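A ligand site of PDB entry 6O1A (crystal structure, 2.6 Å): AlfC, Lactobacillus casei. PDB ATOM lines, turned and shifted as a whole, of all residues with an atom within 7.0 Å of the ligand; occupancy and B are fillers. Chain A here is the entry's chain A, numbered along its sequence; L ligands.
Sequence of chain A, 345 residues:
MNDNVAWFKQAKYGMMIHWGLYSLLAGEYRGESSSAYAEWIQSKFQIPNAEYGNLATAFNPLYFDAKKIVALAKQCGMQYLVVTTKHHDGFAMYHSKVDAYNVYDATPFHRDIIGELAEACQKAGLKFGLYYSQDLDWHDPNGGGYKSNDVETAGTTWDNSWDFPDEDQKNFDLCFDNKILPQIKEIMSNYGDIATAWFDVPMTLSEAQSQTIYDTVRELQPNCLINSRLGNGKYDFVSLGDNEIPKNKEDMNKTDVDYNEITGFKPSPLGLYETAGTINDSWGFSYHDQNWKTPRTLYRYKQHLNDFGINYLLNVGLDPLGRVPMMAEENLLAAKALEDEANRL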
ATOM      1  N   MET A  16       7.394  28.805 -14.027  1.00  0.00           N
ATOM      2  CA  MET A  16       8.287  29.184 -12.901  1.00  0.00           C
ATOM      3  C   MET A  16       9.222  30.263 -13.446  1.00  0.00           C
ATOM      4  O   MET A  16       9.549  30.208 -14.643  1.00  0.00           O
ATOM      5  CB  MET A  16       9.090  27.962 -12.442  1.00  0.00           C
ATOM      6  CG  MET A  16       9.075  27.676 -10.972  1.00  0.00           C
ATOM      7  SD  MET A  16      10.301  28.564 -10.038  1.00  0.00           S
ATOM      8  CE  MET A  16      10.599  27.320  -8.773  1.00  0.00           C
ATOM      9  N   HIS A  18      12.952  32.156 -12.483  1.00  0.00           N
ATOM     10  CA  HIS A  18      14.191  32.525 -11.768  1.00  0.00           C
ATOM     11  C   HIS A  18      14.699  33.841 -12.341  1.00  0.00           C
ATOM     12  O   HIS A  18      14.807  33.933 -13.562  1.00  0.00           O
ATOM     13  CB  HIS A  18      15.247  31.429 -11.868  1.00  0.00           C
ATOM     14  CG  HIS A  18      15.037  30.333 -10.895  1.00  0.00           C
ATOM     15  ND1 HIS A  18      13.978  29.464 -11.004  1.00  0.00           N
ATOM     16  CD2 HIS A  18      15.731  29.958  -9.790  1.00  0.00           C
ATOM     17  CE1 HIS A  18      14.046  28.578 -10.021  1.00  0.00           C
ATOM     18  NE2 HIS A  18      15.113  28.858  -9.262  1.00  0.00           N
ATOM     19  N   TYR A  37      24.053  25.428 -13.013  1.00  0.00           N
ATOM     20  CA  TYR A  37      23.168  26.375 -12.273  1.00  0.00           C
ATOM     21  C   TYR A  37      23.839  27.735 -12.163  1.00  0.00           C
ATOM     22  O   TYR A  37      24.711  27.955 -11.264  1.00  0.00           O
ATOM     23  CB  TYR A  37      22.800  25.806 -10.901  1.00  0.00           C
ATOM     24  CG  TYR A  37      21.884  24.600 -10.917  1.00  0.00           C
ATOM     25  CD1 TYR A  37      21.341  24.106 -12.106  1.00  0.00           C
ATOM     26  CD2 TYR A  37      21.547  23.949  -9.737  1.00  0.00           C
ATOM     27  CE1 TYR A  37      20.508  23.013 -12.125  1.00  0.00           C
ATOM     28  CE2 TYR A  37      20.712  22.844  -9.737  1.00  0.00           C
ATOM     29  CZ  TYR A  37      20.189  22.377 -10.938  1.00  0.00           C
ATOM     30  OH  TYR A  37      19.356  21.293 -10.962  1.00  0.00           O
ATOM     31  N   GLU A  39      22.406  30.517 -11.346  1.00  0.00           N
ATOM     32  CA  GLU A  39      21.885  31.244 -10.171  1.00  0.00           C
ATOM     33  C   GLU A  39      22.790  30.995  -8.963  1.00  0.00           C
ATOM     34  O   GLU A  39      22.781  31.832  -8.065  1.00  0.00           O
ATOM     35  CB  GLU A  39      20.419  30.896  -9.896  1.00  0.00           C
ATOM     36  CG  GLU A  39      20.158  29.477  -9.469  1.00  0.00           C
ATOM     37  CD  GLU A  39      20.175  28.447 -10.571  1.00  0.00           C
ATOM     38  OE1 GLU A  39      20.350  28.823 -11.753  1.00  0.00           O
ATOM     39  OE2 GLU A  39      20.014  27.245 -10.247  1.00  0.00           O
ATOM     40  N   TRP A  40      23.603  29.936  -8.996  1.00  0.00           N
ATOM     41  CA  TRP A  40      24.552  29.554  -7.904  1.00  0.00           C
ATOM     42  C   TRP A  40      25.912  30.232  -8.078  1.00  0.00           C
ATOM     43  O   TRP A  40      26.856  29.834  -7.346  1.00  0.00           O
ATOM     44  CB  TRP A  40      24.710  28.028  -7.856  1.00  0.00           C
ATOM     45  CG  TRP A  40      23.681  27.328  -7.016  1.00  0.00           C
ATOM     46  CD1 TRP A  40      22.390  27.040  -7.357  1.00  0.00           C
ATOM     47  CD2 TRP A  40      23.885  26.784  -5.702  1.00  0.00           C
ATOM     48  NE1 TRP A  40      21.770  26.373  -6.330  1.00  0.00           N
ATOM     49  CE2 TRP A  40      22.662  26.205  -5.306  1.00  0.00           C
ATOM     50  CE3 TRP A  40      24.977  26.756  -4.816  1.00  0.00           C
ATOM     51  CZ2 TRP A  40      22.493  25.617  -4.053  1.00  0.00           C
ATOM     52  CZ3 TRP A  40      24.811  26.167  -3.584  1.00  0.00           C
ATOM     53  CH2 TRP A  40      23.579  25.600  -3.208  1.00  0.00           C
ATOM     54  N   THR A  84      10.698  33.475  -8.065  1.00  0.00           N
ATOM     55  CA  THR A  84      11.734  33.719  -7.038  1.00  0.00           C
ATOM     56  C   THR A  84      11.478  35.081  -6.389  1.00  0.00           C
ATOM     57  O   THR A  84      11.697  36.110  -7.070  1.00  0.00           O
ATOM     58  CB  THR A  84      13.140  33.623  -7.643  1.00  0.00           C
ATOM     59  OG1 THR A  84      13.184  34.495  -8.774  1.00  0.00           O
ATOM     60  CG2 THR A  84      13.503  32.227  -8.083  1.00  0.00           C
ATOM     61  N   HIS A  87      16.274  34.256  -3.684  1.00  0.00           N
ATOM     62  CA  HIS A  87      17.054  33.012  -3.909  1.00  0.00           C
ATOM     63  C   HIS A  87      18.191  32.948  -2.880  1.00  0.00           C
ATOM     64  O   HIS A  87      18.246  33.828  -2.029  1.00  0.00           O
ATOM     65  CB  HIS A  87      17.516  32.945  -5.376  1.00  0.00           C
ATOM     66  CG  HIS A  87      17.672  31.556  -5.866  1.00  0.00           C
ATOM     67  ND1 HIS A  87      18.868  30.868  -5.764  1.00  0.00           N
ATOM     68  CD2 HIS A  87      16.777  30.697  -6.393  1.00  0.00           C
ATOM     69  CE1 HIS A  87      18.707  29.649  -6.237  1.00  0.00           C
ATOM     70  NE2 HIS A  87      17.432  29.517  -6.627  1.00  0.00           N
ATOM     71  N   HIS A  88      19.069  31.954  -2.984  1.00  0.00           N
ATOM     72  CA  HIS A  88      20.210  31.702  -2.047  1.00  0.00           C
ATOM     73  C   HIS A  88      21.069  32.958  -1.837  1.00  0.00           C
ATOM     74  O   HIS A  88      21.637  33.078  -0.726  1.00  0.00           O
ATOM     75  CB  HIS A  88      21.078  30.533  -2.530  1.00  0.00           C
ATOM     76  CG  HIS A  88      20.311  29.289  -2.823  1.00  0.00           C
ATOM     77  ND1 HIS A  88      19.175  28.935  -2.122  1.00  0.00           N
ATOM     78  CD2 HIS A  88      20.531  28.312  -3.725  1.00  0.00           C
ATOM     79  CE1 HIS A  88      18.706  27.795  -2.597  1.00  0.00           C
ATOM     80  NE2 HIS A  88      19.526  27.394  -3.592  1.00  0.00           N
ATOM     81  N   TYR A 131       8.327  31.507  -4.555  1.00  0.00           N
ATOM     82  CA  TYR A 131       9.538  30.779  -4.071  1.00  0.00           C
ATOM     83  C   TYR A 131      10.271  31.701  -3.098  1.00  0.00           C
ATOM     84  O   TYR A 131      10.327  32.912  -3.387  1.00  0.00           O
ATOM     85  CB  TYR A 131      10.431  30.370  -5.245  1.00  0.00           C
ATOM     86  CG  TYR A 131      11.758  29.774  -4.872  1.00  0.00           C
ATOM     87  CD1 TYR A 131      12.782  30.547  -4.357  1.00  0.00           C
ATOM     88  CD2 TYR A 131      12.018  28.439  -5.098  1.00  0.00           C
ATOM     89  CE1 TYR A 131      14.010  29.987  -4.021  1.00  0.00           C
ATOM     90  CE2 TYR A 131      13.242  27.869  -4.802  1.00  0.00           C
ATOM     91  CZ  TYR A 131      14.250  28.651  -4.249  1.00  0.00           C
ATOM     92  OH  TYR A 131      15.451  28.072  -3.929  1.00  0.00           O
ATOM     93  N   LEU A 136      19.115  28.982   3.125  1.00  0.00           N
ATOM     94  CA  LEU A 136      20.338  29.598   2.547  1.00  0.00           C
ATOM     95  C   LEU A 136      20.119  31.092   2.357  1.00  0.00           C
ATOM     96  O   LEU A 136      19.061  31.477   1.810  1.00  0.00           O
ATOM     97  CB  LEU A 136      20.684  28.928   1.208  1.00  0.00           C
ATOM     98  CG  LEU A 136      20.951  27.426   1.260  1.00  0.00           C
ATOM     99  CD1 LEU A 136      21.468  26.924  -0.085  1.00  0.00           C
ATOM    100  CD2 LEU A 136      21.905  27.051   2.385  1.00  0.00           C
ATOM    101  N   ALA A 154      26.167  23.081  -6.345  1.00  0.00           N
ATOM    102  CA  ALA A 154      26.286  23.697  -7.692  1.00  0.00           C
ATOM    103  C   ALA A 154      27.195  24.936  -7.637  1.00  0.00           C
ATOM    104  O   ALA A 154      27.385  25.588  -8.691  1.00  0.00           O
ATOM    105  CB  ALA A 154      24.918  24.037  -8.241  1.00  0.00           C
ATOM    106  N   TRP A 158      27.480  25.544   0.807  1.00  0.00           N
ATOM    107  CA  TRP A 158      26.021  25.857   0.914  1.00  0.00           C
ATOM    108  C   TRP A 158      25.835  27.269   1.467  1.00  0.00           C
ATOM    109  O   TRP A 158      24.893  27.949   1.041  1.00  0.00           O
ATOM    110  CB  TRP A 158      25.313  24.824   1.794  1.00  0.00           C
ATOM    111  CG  TRP A 158      25.256  23.450   1.227  1.00  0.00           C
ATOM    112  CD1 TRP A 158      26.161  22.446   1.397  1.00  0.00           C
ATOM    113  CD2 TRP A 158      24.217  22.909   0.386  1.00  0.00           C
ATOM    114  NE1 TRP A 158      25.767  21.312   0.724  1.00  0.00           N
ATOM    115  CE2 TRP A 158      24.576  21.573   0.096  1.00  0.00           C
ATOM    116  CE3 TRP A 158      23.039  23.422  -0.159  1.00  0.00           C
ATOM    117  CZ2 TRP A 158      23.794  20.754  -0.711  1.00  0.00           C
ATOM    118  CZ3 TRP A 158      22.265  22.608  -0.956  1.00  0.00           C
ATOM    119  CH2 TRP A 158      22.632  21.291  -1.232  1.00  0.00           C
ATOM    120  N   TRP A 198       6.621  27.823  -2.193  1.00  0.00           N
ATOM    121  CA  TRP A 198       7.767  26.986  -2.652  1.00  0.00           C
ATOM    122  C   TRP A 198       8.992  27.292  -1.801  1.00  0.00           C
ATOM    123  O   TRP A 198       9.604  28.339  -2.012  1.00  0.00           O
ATOM    124  CB  TRP A 198       8.005  27.276  -4.134  1.00  0.00           C
ATOM    125  CG  TRP A 198       8.078  26.084  -5.034  1.00  0.00           C
ATOM    126  CD1 TRP A 198       7.042  25.506  -5.715  1.00  0.00           C
ATOM    127  CD2 TRP A 198       9.263  25.362  -5.388  1.00  0.00           C
ATOM    128  NE1 TRP A 198       7.511  24.452  -6.465  1.00  0.00           N
ATOM    129  CE2 TRP A 198       8.870  24.343  -6.286  1.00  0.00           C
ATOM    130  CE3 TRP A 198      10.615  25.458  -5.023  1.00  0.00           C
ATOM    131  CZ2 TRP A 198       9.787  23.439  -6.826  1.00  0.00           C
ATOM    132  CZ3 TRP A 198      11.511  24.575  -5.566  1.00  0.00           C
ATOM    133  CH2 TRP A 198      11.105  23.582  -6.458  1.00  0.00           C
ATOM    134  N   PHE A 199       9.325  26.422  -0.851  1.00  0.00           N
ATOM    135  CA  PHE A 199      10.495  26.561   0.048  1.00  0.00           C
ATOM    136  C   PHE A 199      11.575  25.574  -0.373  1.00  0.00           C
ATOM    137  O   PHE A 199      11.285  24.694  -1.205  1.00  0.00           O
ATOM    138  CB  PHE A 199      10.039  26.395   1.507  1.00  0.00           C
ATOM    139  CG  PHE A 199       9.117  27.479   1.981  1.00  0.00           C
ATOM    140  CD1 PHE A 199       9.620  28.721   2.371  1.00  0.00           C
ATOM    141  CD2 PHE A 199       7.744  27.296   1.995  1.00  0.00           C
ATOM    142  CE1 PHE A 199       8.763  29.735   2.779  1.00  0.00           C
ATOM    143  CE2 PHE A 199       6.895  28.298   2.423  1.00  0.00           C
ATOM    144  CZ  PHE A 199       7.399  29.517   2.814  1.00  0.00           C
ATOM    145  N   ASP A 200      12.791  25.735   0.152  1.00  0.00           N
ATOM    146  CA  ASP A 200      13.921  24.796  -0.057  1.00  0.00           C
ATOM    147  C   ASP A 200      13.878  23.733   1.018  1.00  0.00           C
ATOM    148  O   ASP A 200      13.082  23.895   1.952  1.00  0.00           O
ATOM    149  CB  ASP A 200      15.260  25.528  -0.091  1.00  0.00           C
ATOM    150  CG  ASP A 200      15.525  26.117  -1.467  1.00  0.00           C
ATOM    151  OD1 ASP A 200      15.868  25.330  -2.397  1.00  0.00           O
ATOM    152  OD2 ASP A 200      15.370  27.356  -1.622  1.00  0.00           O
ATOM    153  N   VAL A 201      14.674  22.664   0.884  1.00  0.00           N
ATOM    154  CA  VAL A 201      14.820  21.635   1.959  1.00  0.00           C
ATOM    155  C   VAL A 201      15.681  22.274   3.040  1.00  0.00           C
ATOM    156  O   VAL A 201      16.730  22.860   2.739  1.00  0.00           O
ATOM    157  CB  VAL A 201      15.405  20.301   1.487  1.00  0.00           C
ATOM    158  CG1 VAL A 201      14.656  19.748   0.273  1.00  0.00           C
ATOM    159  CG2 VAL A 201      16.910  20.364   1.214  1.00  0.00           C
ATOM    160  N   ARG A 229       9.003  20.336   0.327  1.00  0.00           N
ATOM    161  CA  ARG A 229      10.401  20.741   0.632  1.00  0.00           C
ATOM    162  C   ARG A 229      10.497  21.377   2.016  1.00  0.00           C
ATOM    163  O   ARG A 229      11.541  21.152   2.668  1.00  0.00           O
ATOM    164  CB  ARG A 229      10.934  21.710  -0.426  1.00  0.00           C
ATOM    165  CG  ARG A 229      11.029  21.117  -1.813  1.00  0.00           C
ATOM    166  CD  ARG A 229      12.406  21.315  -2.424  1.00  0.00           C
ATOM    167  NE  ARG A 229      12.386  21.326  -3.875  1.00  0.00           N
ATOM    168  CZ  ARG A 229      12.806  20.340  -4.670  1.00  0.00           C
ATOM    169  NH1 ARG A 229      13.292  19.218  -4.156  1.00  0.00           N
ATOM    170  NH2 ARG A 229      12.750  20.485  -5.982  1.00  0.00           N
ATOM    171  N   ALA A 276       9.086  20.236 -11.070  1.00  0.00           N
ATOM    172  CA  ALA A 276       9.659  21.446 -11.689  1.00  0.00           C
ATOM    173  C   ALA A 276      10.813  21.029 -12.608  1.00  0.00           C
ATOM    174  O   ALA A 276      11.512  20.065 -12.263  1.00  0.00           O
ATOM    175  CB  ALA A 276      10.126  22.414 -10.635  1.00  0.00           C
ATOM    176  N   TRP A 283      18.568  27.148 -14.179  1.00  0.00           N
ATOM    177  CA  TRP A 283      17.344  27.835 -13.662  1.00  0.00           C
ATOM    178  C   TRP A 283      17.481  29.325 -13.941  1.00  0.00           C
ATOM    179  O   TRP A 283      16.572  29.895 -14.566  1.00  0.00           O
ATOM    180  CB  TRP A 283      17.116  27.536 -12.173  1.00  0.00           C
ATOM    181  CG  TRP A 283      16.913  26.076 -11.944  1.00  0.00           C
ATOM    182  CD1 TRP A 283      17.859  25.138 -11.653  1.00  0.00           C
ATOM    183  CD2 TRP A 283      15.672  25.366 -12.056  1.00  0.00           C
ATOM    184  NE1 TRP A 283      17.284  23.896 -11.548  1.00  0.00           N
ATOM    185  CE2 TRP A 283      15.942  24.017 -11.788  1.00  0.00           C
ATOM    186  CE3 TRP A 283      14.358  25.752 -12.334  1.00  0.00           C
ATOM    187  CZ2 TRP A 283      14.947  23.041 -11.782  1.00  0.00           C
ATOM    188  CZ3 TRP A 283      13.371  24.798 -12.328  1.00  0.00           C
ATOM    189  CH2 TRP A 283      13.659  23.456 -12.049  1.00  0.00           C
ATOM    190  N   GLY A 284      18.600  29.920 -13.521  1.00  0.00           N
ATOM    191  CA  GLY A 284      18.958  31.298 -13.898  1.00  0.00           C
ATOM    192  C   GLY A 284      19.411  31.343 -15.348  1.00  0.00           C
ATOM    193  O   GLY A 284      19.992  30.354 -15.816  1.00  0.00           O
ATOM    194  N   ASN A 315      10.311  26.131 -15.847  1.00  0.00           N
ATOM    195  CA  ASN A 315      11.049  27.372 -15.476  1.00  0.00           C
ATOM    196  C   ASN A 315      11.516  28.141 -16.711  1.00  0.00           C
ATOM    197  O   ASN A 315      12.080  27.543 -17.650  1.00  0.00           O
ATOM    198  CB  ASN A 315      12.248  27.087 -14.580  1.00  0.00           C
ATOM    199  CG  ASN A 315      13.059  28.329 -14.313  1.00  0.00           C
ATOM    200  OD1 ASN A 315      12.711  29.100 -13.411  1.00  0.00           O
ATOM    201  ND2 ASN A 315      14.159  28.509 -15.039  1.00  0.00           N
HETATM  202  C1  LIG L   1      17.295  24.022  -6.033  1.00  0.00           C
HETATM  203  C2  LIG L   1      18.055  25.334  -6.031  1.00  0.00           C
HETATM  204  O1  LIG L   1      19.343  25.110  -5.397  1.00  0.00           O
HETATM  205  C3  LIG L   1      18.217  25.844  -7.427  1.00  0.00           C
HETATM  206  O2  LIG L   1      18.975  27.083  -7.455  1.00  0.00           O
HETATM  207  C4  LIG L   1      16.872  26.054  -8.087  1.00  0.00           C
HETATM  208  O3  LIG L   1      16.183  27.142  -7.461  1.00  0.00           O
HETATM  209  C5  LIG L   1      16.012  24.774  -8.030  1.00  0.00           C
HETATM  210  C6  LIG L   1      14.615  25.053  -8.481  1.00  0.00           C
HETATM  211  O4  LIG L   1      15.947  24.146  -6.703  1.00  0.00           O
HETATM  212  O5  LIG L   1      17.130  23.611  -4.749  1.00  0.00           O
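An oxygen (O1) of the ligand lies within hydrogen-bond range of a ring nitrogen (NE2) of His 88. The side-chain carboxylate (OE2) of Glu 39 is in hydrogen-bond range of an oxygen (O2) of the ligand, 3.0 Å away. The side-chain carboxylate of Asp 200 lies within hydrogen-bond range of an oxygen (O5) of the ligand (3.2 Å). An oxygen (O1) of the ligand is in hydrogen-bond range of the indole nitrogen of Trp 40 (2.9 Å). O3 of the ligand sits at hydrogen-bond distance from NE2 of His 18 (2.7 Å). A ring nitrogen (NE2) of His 87 sits at hydrogen-bond distance from an oxygen (O3) of the ligand (2.8 Å).
The side-chain carboxylate (OD2) of Asp 200 is in hydrogen-bond range of the side-chain hydroxyl (OH) of Tyr 131, at 2.4 Å. OE1 of Glu 39 sits at hydrogen-bond distance from N of Trp 283, 3.4 Å away. The indole nitrogen of Trp 283 sits close to the side-chain hydroxyl of Tyr 37 (3.4 Å). The side-chain carboxylate (OE1) of Glu 39 is in hydrogen-bond range of the backbone NH (N) of Gly 284, 2.7 Å away. ND1 of His 18 sits at hydrogen-bond distance from OD1 of Asn 315 (2.7 Å). The side-chain amide nitrogen (ND2) of Asn 315 lies within hydrogen-bond range of the backbone carbonyl oxygen (O) of Trp 283 (2.8 Å).
Residues that only touch the ligand: Trp 283 (3.7 Å) and Tyr 131 (3.7 Å).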
